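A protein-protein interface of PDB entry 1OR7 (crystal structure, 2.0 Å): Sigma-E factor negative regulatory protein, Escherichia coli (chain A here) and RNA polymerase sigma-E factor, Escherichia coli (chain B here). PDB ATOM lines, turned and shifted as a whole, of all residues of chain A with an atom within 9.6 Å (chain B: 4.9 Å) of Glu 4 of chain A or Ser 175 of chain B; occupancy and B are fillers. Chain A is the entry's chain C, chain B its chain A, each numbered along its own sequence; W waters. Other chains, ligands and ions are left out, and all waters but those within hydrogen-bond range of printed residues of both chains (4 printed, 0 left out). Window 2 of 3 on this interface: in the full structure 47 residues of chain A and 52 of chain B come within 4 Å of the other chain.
OG of Ser 175 of chain B sits at hydrogen-bond distance from OE2 of Glu 4 of chain A, 2.7 Å away.
The backbone NH (N) of Glu 13 of chain A lies within hydrogen-bond range of the backbone carbonyl oxygen (O) of Ala 8 of chain A (3.0 Å).
Among the printed residues, merely in contact across the chains: Glu 4 of chain A with Arg 174 of chain B (3.3 Å), Tyr 36 of chain A with Phe 178 of chain B (3.4 Å), Lys 3 of chain A with Phe 178 of chain B (3.5 Å), Ser 7 of chain A with Phe 178 of chain B (3.6 Å), Ala 8 of chain A with Arg 174 of chain B (3.6 Å), Glu 4 of chain A with Phe 178 of chain B (3.7 Å) and Asp 11 of chain A with Ile 177 of chain B (3.9 Å).
Printed residues of chain B within 4 Å of Glu 4 of chain A: Arg 174 (3.3 Å), Ser 175 (2.7 Å) and Phe 178 (3.7 Å).
Gln 5 of chain A touches none of the printed residues of chain B.
Leu 6 of chain A touches none of the printed residues of chain B.
Of the printed residues of chain B, Ala 8 of chain A touches Arg 174.
Of the printed residues of chain B, Tyr 36 of chain A touches Phe 178 (3.4 Å).
Of chain A, only Glu 4 comes within 4 Å of Ser 175 of chain B.
Phe 178 of chain B touches four residues of chain A.
The nearest printed residue of chain B that does not touch Glu 4 of chain A is Gly 171 of chain B (4.6 Å).
The nearest residue of chain A that does not touch Ser 175 of chain B is Ser 7 of chain A (6.8 Å).
Among the printed residues, 8 pairs touch across the chains.
Water W1 lies within hydrogen-bond range of OE2 of Glu 4 of chain A (2.5 Å), OG of Ser 175 of chain B (3.0 Å) and O of Gly 171 of chain B (3.2 Å).
Water W2 bridges OG of Ser 7 of chain A (2.6 Å) and O of Arg 174 of chain B (2.8 Å).
Water W3 lies within hydrogen-bond range of OE1 of Glu 4 of chain A, OG of Ser 175 of chain B and NH2 of Arg 179 of chain B.
Water W4 bridges the side-chain carboxylate of Glu 4 of chain A (3.1 Å) and the guanidinium group of Arg 179 of chain B (3.2 Å).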
ATOM      1  N   MET A   1      34.651  20.504 -26.801  1.00  0.00           N
ATOM      2  CA  MET A   1      33.577  20.247 -25.815  1.00  0.00           C
ATOM      3  C   MET A   1      32.607  19.207 -26.355  1.00  0.00           C
ATOM      4  O   MET A   1      32.324  19.173 -27.547  1.00  0.00           O
ATOM      5  CB  MET A   1      32.840  21.554 -25.523  1.00  0.00           C
ATOM      6  CG  MET A   1      31.444  21.415 -24.973  1.00  0.00           C
ATOM      7  SD  MET A   1      30.652  23.207 -24.685  1.00  0.00           S
ATOM      8  CE  MET A   1      30.382  23.201 -22.766  1.00  0.00           C
ATOM      9  N   GLN A   2      32.136  18.326 -25.483  1.00  0.00           N
ATOM     10  CA  GLN A   2      31.102  17.374 -25.867  1.00  0.00           C
ATOM     11  C   GLN A   2      29.714  17.886 -25.512  1.00  0.00           C
ATOM     12  O   GLN A   2      29.531  18.650 -24.568  1.00  0.00           O
ATOM     13  CB  GLN A   2      31.339  16.030 -25.176  1.00  0.00           C
ATOM     14  CG  GLN A   2      32.708  15.407 -25.476  1.00  0.00           C
ATOM     15  CD  GLN A   2      32.812  14.869 -26.903  1.00  0.00           C
ATOM     16  OE1 GLN A   2      32.363  13.748 -27.188  1.00  0.00           O
ATOM     17  NE2 GLN A   2      33.407  15.664 -27.800  1.00  0.00           N
ATOM     18  N   LYS A   3      28.729  17.431 -26.272  1.00  0.00           N
ATOM     19  CA  LYS A   3      27.350  17.752 -26.000  1.00  0.00           C
ATOM     20  C   LYS A   3      26.967  17.307 -24.588  1.00  0.00           C
ATOM     21  O   LYS A   3      26.176  17.976 -23.936  1.00  0.00           O
ATOM     22  CB  LYS A   3      26.424  17.111 -27.039  1.00  0.00           C
ATOM     23  CG  LYS A   3      26.486  17.777 -28.402  1.00  0.00           C
ATOM     24  CD  LYS A   3      25.507  17.171 -29.423  1.00  0.00           C
ATOM     25  CE  LYS A   3      25.603  17.935 -30.772  1.00  0.00           C
ATOM     26  NZ  LYS A   3      24.861  17.308 -31.908  1.00  0.00           N
ATOM     27  N   GLU A   4      27.541  16.212 -24.097  1.00  0.00           N
ATOM     28  CA  GLU A   4      27.208  15.759 -22.754  1.00  0.00           C
ATOM     29  C   GLU A   4      27.580  16.834 -21.707  1.00  0.00           C
ATOM     30  O   GLU A   4      26.871  17.032 -20.720  1.00  0.00           O
ATOM     31  CB  GLU A   4      27.873  14.401 -22.433  1.00  0.00           C
ATOM     32  CG  GLU A   4      27.456  13.838 -21.082  1.00  0.00           C
ATOM     33  CD  GLU A   4      27.846  12.379 -20.881  1.00  0.00           C
ATOM     34  OE1 GLU A   4      27.795  11.574 -21.836  1.00  0.00           O
ATOM     35  OE2 GLU A   4      28.190  12.028 -19.750  1.00  0.00           O
ATOM     36  N   GLN A   5      28.682  17.528 -21.947  1.00  0.00           N
ATOM     37  CA  GLN A   5      29.137  18.606 -21.090  1.00  0.00           C
ATOM     38  C   GLN A   5      28.162  19.766 -21.212  1.00  0.00           C
ATOM     39  O   GLN A   5      27.829  20.423 -20.223  1.00  0.00           O
ATOM     40  CB  GLN A   5      30.563  19.049 -21.488  1.00  0.00           C
ATOM     41  CG  GLN A   5      31.613  17.983 -21.254  1.00  0.00           C
ATOM     42  CD  GLN A   5      33.026  18.448 -21.638  1.00  0.00           C
ATOM     43  OE1 GLN A   5      33.279  18.817 -22.784  1.00  0.00           O
ATOM     44  NE2 GLN A   5      33.921  18.451 -20.677  1.00  0.00           N
ATOM     45  N   LEU A   6      27.705  20.031 -22.427  1.00  0.00           N
ATOM     46  CA  LEU A   6      26.684  21.057 -22.629  1.00  0.00           C
ATOM     47  C   LEU A   6      25.416  20.714 -21.834  1.00  0.00           C
ATOM     48  O   LEU A   6      24.817  21.562 -21.168  1.00  0.00           O
ATOM     49  CB  LEU A   6      26.406  21.174 -24.129  1.00  0.00           C
ATOM     50  CG  LEU A   6      25.436  22.190 -24.698  1.00  0.00           C
ATOM     51  CD1 LEU A   6      25.284  23.337 -23.800  1.00  0.00           C
ATOM     52  CD2 LEU A   6      25.959  22.690 -26.034  1.00  0.00           C
ATOM     53  N   SER A   7      25.012  19.453 -21.900  1.00  0.00           N
ATOM     54  CA  SER A   7      23.875  18.973 -21.137  1.00  0.00           C
ATOM     55  C   SER A   7      24.082  19.235 -19.647  1.00  0.00           C
ATOM     56  O   SER A   7      23.189  19.700 -18.966  1.00  0.00           O
ATOM     57  CB  SER A   7      23.704  17.476 -21.347  1.00  0.00           C
ATOM     58  OG  SER A   7      22.461  17.035 -20.863  1.00  0.00           O
ATOM     59  N   ALA A   8      25.248  18.904 -19.119  1.00  0.00           N
ATOM     60  CA  ALA A   8      25.498  19.167 -17.698  1.00  0.00           C
ATOM     61  C   ALA A   8      25.464  20.661 -17.360  1.00  0.00           C
ATOM     62  O   ALA A   8      24.889  21.081 -16.333  1.00  0.00           O
ATOM     63  CB  ALA A   8      26.821  18.516 -17.239  1.00  0.00           C
ATOM     64  N   LEU A   9      26.064  21.475 -18.227  1.00  0.00           N
ATOM     65  CA  LEU A   9      26.087  22.919 -18.025  1.00  0.00           C
ATOM     66  C   LEU A   9      24.672  23.539 -17.925  1.00  0.00           C
ATOM     67  O   LEU A   9      24.375  24.313 -17.032  1.00  0.00           O
ATOM     68  CB  LEU A   9      26.823  23.540 -19.195  1.00  0.00           C
ATOM     69  CG  LEU A   9      27.123  25.020 -19.134  1.00  0.00           C
ATOM     70  CD1 LEU A   9      28.191  25.271 -18.102  1.00  0.00           C
ATOM     71  CD2 LEU A   9      27.580  25.477 -20.518  1.00  0.00           C
ATOM     72  N   MET A  10      23.785  23.174 -18.820  1.00  0.00           N
ATOM     73  CA  MET A  10      22.448  23.764 -18.796  1.00  0.00           C
ATOM     74  C   MET A  10      21.662  23.335 -17.547  1.00  0.00           C
ATOM     75  O   MET A  10      20.642  23.933 -17.224  1.00  0.00           O
ATOM     76  CB  MET A  10      21.683  23.372 -20.020  1.00  0.00           C
ATOM     77  CG  MET A  10      20.960  22.100 -19.779  1.00  0.00           C
ATOM     78  SD  MET A  10      20.037  21.713 -21.343  1.00  0.00           S
ATOM     79  CE  MET A  10      18.298  22.722 -21.114  1.00  0.00           C
ATOM     80  N   ASP A  11      22.157  22.323 -16.844  1.00  0.00           N
ATOM     81  CA  ASP A  11      21.529  21.861 -15.617  1.00  0.00           C
ATOM     82  C   ASP A  11      22.205  22.426 -14.358  1.00  0.00           C
ATOM     83  O   ASP A  11      21.857  22.059 -13.230  1.00  0.00           O
ATOM     84  CB  ASP A  11      21.608  20.346 -15.543  1.00  0.00           C
ATOM     85  CG  ASP A  11      20.590  19.647 -16.424  1.00  0.00           C
ATOM     86  OD1 ASP A  11      19.480  20.205 -16.658  1.00  0.00           O
ATOM     87  OD2 ASP A  11      20.820  18.507 -16.887  1.00  0.00           O
ATOM     88  N   GLY A  12      23.205  23.257 -14.556  1.00  0.00           N
ATOM     89  CA  GLY A  12      23.908  23.872 -13.449  1.00  0.00           C
ATOM     90  C   GLY A  12      24.830  22.900 -12.771  1.00  0.00           C
ATOM     91  O   GLY A  12      25.314  23.158 -11.673  1.00  0.00           O
ATOM     92  N   GLU A  13      25.089  21.785 -13.431  1.00  0.00           N
ATOM     93  CA  GLU A  13      25.838  20.733 -12.800  1.00  0.00           C
ATOM     94  C   GLU A  13      27.333  20.876 -13.050  1.00  0.00           C
ATOM     95  O   GLU A  13      28.105  20.168 -12.452  1.00  0.00           O
ATOM     96  CB  GLU A  13      25.315  19.372 -13.232  1.00  0.00           C
ATOM     97  CG  GLU A  13      23.893  19.109 -12.732  1.00  0.00           C
ATOM     98  CD  GLU A  13      23.819  18.680 -11.262  1.00  0.00           C
ATOM     99  OE1 GLU A  13      24.843  18.280 -10.707  1.00  0.00           O
ATOM    100  OE2 GLU A  13      22.725  18.754 -10.662  1.00  0.00           O
ATOM    101  N   THR A  14      27.727  21.759 -13.959  1.00  0.00           N
ATOM    102  CA  THR A  14      29.112  22.187 -14.070  1.00  0.00           C
ATOM    103  C   THR A  14      29.045  23.667 -14.360  1.00  0.00           C
ATOM    104  O   THR A  14      28.134  24.126 -15.037  1.00  0.00           O
ATOM    105  CB  THR A  14      29.905  21.478 -15.161  1.00  0.00           C
ATOM    106  OG1 THR A  14      31.169  22.136 -15.288  1.00  0.00           O
ATOM    107  CG2 THR A  14      29.302  21.652 -16.541  1.00  0.00           C
ATOM    108  N   LEU A  19      34.216  25.855 -20.340  1.00  0.00           N
ATOM    109  CA  LEU A  19      33.088  25.311 -21.064  1.00  0.00           C
ATOM    110  C   LEU A  19      32.158  26.444 -21.465  1.00  0.00           C
ATOM    111  O   LEU A  19      31.667  26.483 -22.581  1.00  0.00           O
ATOM    112  CB  LEU A  19      32.369  24.243 -20.242  1.00  0.00           C
ATOM    113  CG  LEU A  19      33.043  22.859 -20.189  1.00  0.00           C
ATOM    114  CD1 LEU A  19      33.101  22.099 -21.524  1.00  0.00           C
ATOM    115  CD2 LEU A  19      34.416  22.977 -19.699  1.00  0.00           C
ATOM    116  N   MET A  29      27.538  24.069 -30.711  1.00  0.00           N
ATOM    117  CA  MET A  29      27.118  24.010 -29.329  1.00  0.00           C
ATOM    118  C   MET A  29      26.002  25.029 -29.118  1.00  0.00           C
ATOM    119  O   MET A  29      25.102  24.783 -28.359  1.00  0.00           O
ATOM    120  CB  MET A  29      28.289  24.270 -28.366  1.00  0.00           C
ATOM    121  CG  MET A  29      29.351  23.147 -28.302  1.00  0.00           C
ATOM    122  SD  MET A  29      28.635  21.352 -27.855  1.00  0.00           S
ATOM    123  CE  MET A  29      27.962  20.745 -29.653  1.00  0.00           C
ATOM    124  N   THR A  32      22.797  23.444 -30.066  1.00  0.00           N
ATOM    125  CA  THR A  32      22.397  22.469 -29.063  1.00  0.00           C
ATOM    126  C   THR A  32      21.836  23.163 -27.826  1.00  0.00           C
ATOM    127  O   THR A  32      20.803  22.747 -27.278  1.00  0.00           O
ATOM    128  CB  THR A  32      23.605  21.601 -28.730  1.00  0.00           C
ATOM    129  OG1 THR A  32      24.077  20.971 -29.938  1.00  0.00           O
ATOM    130  CG2 THR A  32      23.230  20.492 -27.820  1.00  0.00           C
ATOM    131  N   TYR A  36      18.118  22.188 -26.742  1.00  0.00           N
ATOM    132  CA  TYR A  36      17.866  21.599 -25.419  1.00  0.00           C
ATOM    133  C   TYR A  36      16.992  22.501 -24.538  1.00  0.00           C
ATOM    134  O   TYR A  36      16.179  22.005 -23.770  1.00  0.00           O
ATOM    135  CB  TYR A  36      19.175  21.251 -24.671  1.00  0.00           C
ATOM    136  CG  TYR A  36      19.984  20.082 -25.222  1.00  0.00           C
ATOM    137  CD1 TYR A  36      19.560  19.339 -26.324  1.00  0.00           C
ATOM    138  CD2 TYR A  36      21.217  19.744 -24.659  1.00  0.00           C
ATOM    139  CE1 TYR A  36      20.336  18.282 -26.835  1.00  0.00           C
ATOM    140  CE2 TYR A  36      21.988  18.681 -25.161  1.00  0.00           C
ATOM    141  CZ  TYR A  36      21.536  17.964 -26.234  1.00  0.00           C
ATOM    142  OH  TYR A  36      22.303  16.923 -26.700  1.00  0.00           O
ATOM    143  N   GLY B 171      27.510  10.258 -12.571  1.00  0.00           N
ATOM    144  CA  GLY B 171      27.965  10.174 -13.948  1.00  0.00           C
ATOM    145  C   GLY B 171      26.922   9.479 -14.815  1.00  0.00           C
ATOM    146  O   GLY B 171      26.726   9.810 -15.971  1.00  0.00           O
ATOM    147  N   THR B 172      26.237   8.503 -14.249  1.00  0.00           N
ATOM    148  CA  THR B 172      25.210   7.807 -14.986  1.00  0.00           C
ATOM    149  C   THR B 172      23.988   8.710 -15.151  1.00  0.00           C
ATOM    150  O   THR B 172      23.371   8.744 -16.201  1.00  0.00           O
ATOM    151  CB  THR B 172      24.922   6.483 -14.268  1.00  0.00           C
ATOM    152  OG1 THR B 172      26.160   5.785 -14.132  1.00  0.00           O
ATOM    153  CG2 THR B 172      24.099   5.537 -15.123  1.00  0.00           C
ATOM    154  N   VAL B 173      23.654   9.495 -14.142  1.00  0.00           N
ATOM    155  CA  VAL B 173      22.540  10.419 -14.296  1.00  0.00           C
ATOM    156  C   VAL B 173      22.855  11.392 -15.403  1.00  0.00           C
ATOM    157  O   VAL B 173      22.021  11.672 -16.265  1.00  0.00           O
ATOM    158  CB  VAL B 173      22.260  11.190 -13.024  1.00  0.00           C
ATOM    159  CG1 VAL B 173      21.160  12.159 -13.257  1.00  0.00           C
ATOM    160  CG2 VAL B 173      21.847  10.245 -11.934  1.00  0.00           C
ATOM    161  N   ARG B 174      24.081  11.883 -15.413  1.00  0.00           N
ATOM    162  CA  ARG B 174      24.439  12.862 -16.416  1.00  0.00           C
ATOM    163  C   ARG B 174      24.236  12.284 -17.797  1.00  0.00           C
ATOM    164  O   ARG B 174      23.652  12.927 -18.681  1.00  0.00           O
ATOM    165  CB  ARG B 174      25.885  13.324 -16.266  1.00  0.00           C
ATOM    166  CG  ARG B 174      26.331  14.256 -17.400  1.00  0.00           C
ATOM    167  CD  ARG B 174      27.854  14.488 -17.530  1.00  0.00           C
ATOM    168  NE  ARG B 174      28.409  15.323 -16.476  1.00  0.00           N
ATOM    169  CZ  ARG B 174      29.483  16.106 -16.617  1.00  0.00           C
ATOM    170  NH1 ARG B 174      30.192  16.118 -17.745  1.00  0.00           N
ATOM    171  NH2 ARG B 174      29.872  16.864 -15.608  1.00  0.00           N
ATOM    172  N   SER B 175      24.748  11.085 -17.990  1.00  0.00           N
ATOM    173  CA  SER B 175      24.666  10.453 -19.276  1.00  0.00           C
ATOM    174  C   SER B 175      23.229  10.121 -19.686  1.00  0.00           C
ATOM    175  O   SER B 175      22.881  10.249 -20.837  1.00  0.00           O
ATOM    176  CB  SER B 175      25.566   9.229 -19.304  1.00  0.00           C
ATOM    177  OG  SER B 175      26.909   9.661 -19.523  1.00  0.00           O
ATOM    178  N   ARG B 176      22.389   9.738 -18.733  1.00  0.00           N
ATOM    179  CA  ARG B 176      21.027   9.378 -19.050  1.00  0.00           C
ATOM    180  C   ARG B 176      20.242  10.590 -19.503  1.00  0.00           C
ATOM    181  O   ARG B 176      19.502  10.524 -20.483  1.00  0.00           O
ATOM    182  CB  ARG B 176      20.335   8.739 -17.846  1.00  0.00           C
ATOM    183  CG  ARG B 176      20.689   7.287 -17.630  1.00  0.00           C
ATOM    184  CD  ARG B 176      20.084   6.740 -16.376  1.00  0.00           C
ATOM    185  NE  ARG B 176      20.548   5.405 -16.146  1.00  0.00           N
ATOM    186  CZ  ARG B 176      20.384   4.739 -15.023  1.00  0.00           C
ATOM    187  NH1 ARG B 176      19.783   5.281 -13.981  1.00  0.00           N
ATOM    188  NH2 ARG B 176      20.852   3.521 -14.942  1.00  0.00           N
ATOM    189  N   ILE B 177      20.411  11.705 -18.800  1.00  0.00           N
ATOM    190  CA  ILE B 177      19.720  12.902 -19.184  1.00  0.00           C
ATOM    191  C   ILE B 177      20.191  13.363 -20.564  1.00  0.00           C
ATOM    192  O   ILE B 177      19.387  13.782 -21.410  1.00  0.00           O
ATOM    193  CB  ILE B 177      19.892  13.978 -18.115  1.00  0.00           C
ATOM    194  CG1 ILE B 177      19.170  13.524 -16.847  1.00  0.00           C
ATOM    195  CG2 ILE B 177      19.343  15.333 -18.603  1.00  0.00           C
ATOM    196  CD1 ILE B 177      19.541  14.321 -15.646  1.00  0.00           C
ATOM    197  N   PHE B 178      21.494  13.280 -20.810  1.00  0.00           N
ATOM    198  CA  PHE B 178      22.022  13.666 -22.120  1.00  0.00           C
ATOM    199  C   PHE B 178      21.385  12.836 -23.247  1.00  0.00           C
ATOM    200  O   PHE B 178      20.895  13.377 -24.266  1.00  0.00           O
ATOM    201  CB  PHE B 178      23.532  13.491 -22.137  1.00  0.00           C
ATOM    202  CG  PHE B 178      24.132  13.503 -23.507  1.00  0.00           C
ATOM    203  CD1 PHE B 178      23.956  14.586 -24.343  1.00  0.00           C
ATOM    204  CD2 PHE B 178      24.890  12.444 -23.945  1.00  0.00           C
ATOM    205  CE1 PHE B 178      24.520  14.606 -25.604  1.00  0.00           C
ATOM    206  CE2 PHE B 178      25.443  12.450 -25.201  1.00  0.00           C
ATOM    207  CZ  PHE B 178      25.252  13.534 -26.036  1.00  0.00           C
ATOM    208  N   ARG B 179      21.390  11.516 -23.069  1.00  0.00           N
ATOM    209  CA  ARG B 179      20.873  10.645 -24.121  1.00  0.00           C
ATOM    210  C   ARG B 179      19.377  10.848 -24.352  1.00  0.00           C
ATOM    211  O   ARG B 179      18.923  10.723 -25.443  1.00  0.00           O
ATOM    212  CB  ARG B 179      21.196   9.186 -23.812  1.00  0.00           C
ATOM    213  CG  ARG B 179      22.682   8.918 -23.822  1.00  0.00           C
ATOM    214  CD  ARG B 179      23.291   8.932 -25.200  1.00  0.00           C
ATOM    215  NE  ARG B 179      24.735   8.891 -25.104  1.00  0.00           N
ATOM    216  CZ  ARG B 179      25.567   9.083 -26.114  1.00  0.00           C
ATOM    217  NH1 ARG B 179      25.099   9.353 -27.333  1.00  0.00           N
ATOM    218  NH2 ARG B 179      26.877   9.018 -25.893  1.00  0.00           N
HETATM  219  O   HOH W   1      29.176  10.674 -17.851  1.00  0.00           O
HETATM  220  O   HOH W   2      23.213  15.648 -18.823  1.00  0.00           O
HETATM  221  O   HOH W   3      26.957   9.090 -22.675  1.00  0.00           O
HETATM  222  O   HOH W   4      28.860  11.246 -24.708  1.00  0.00           O
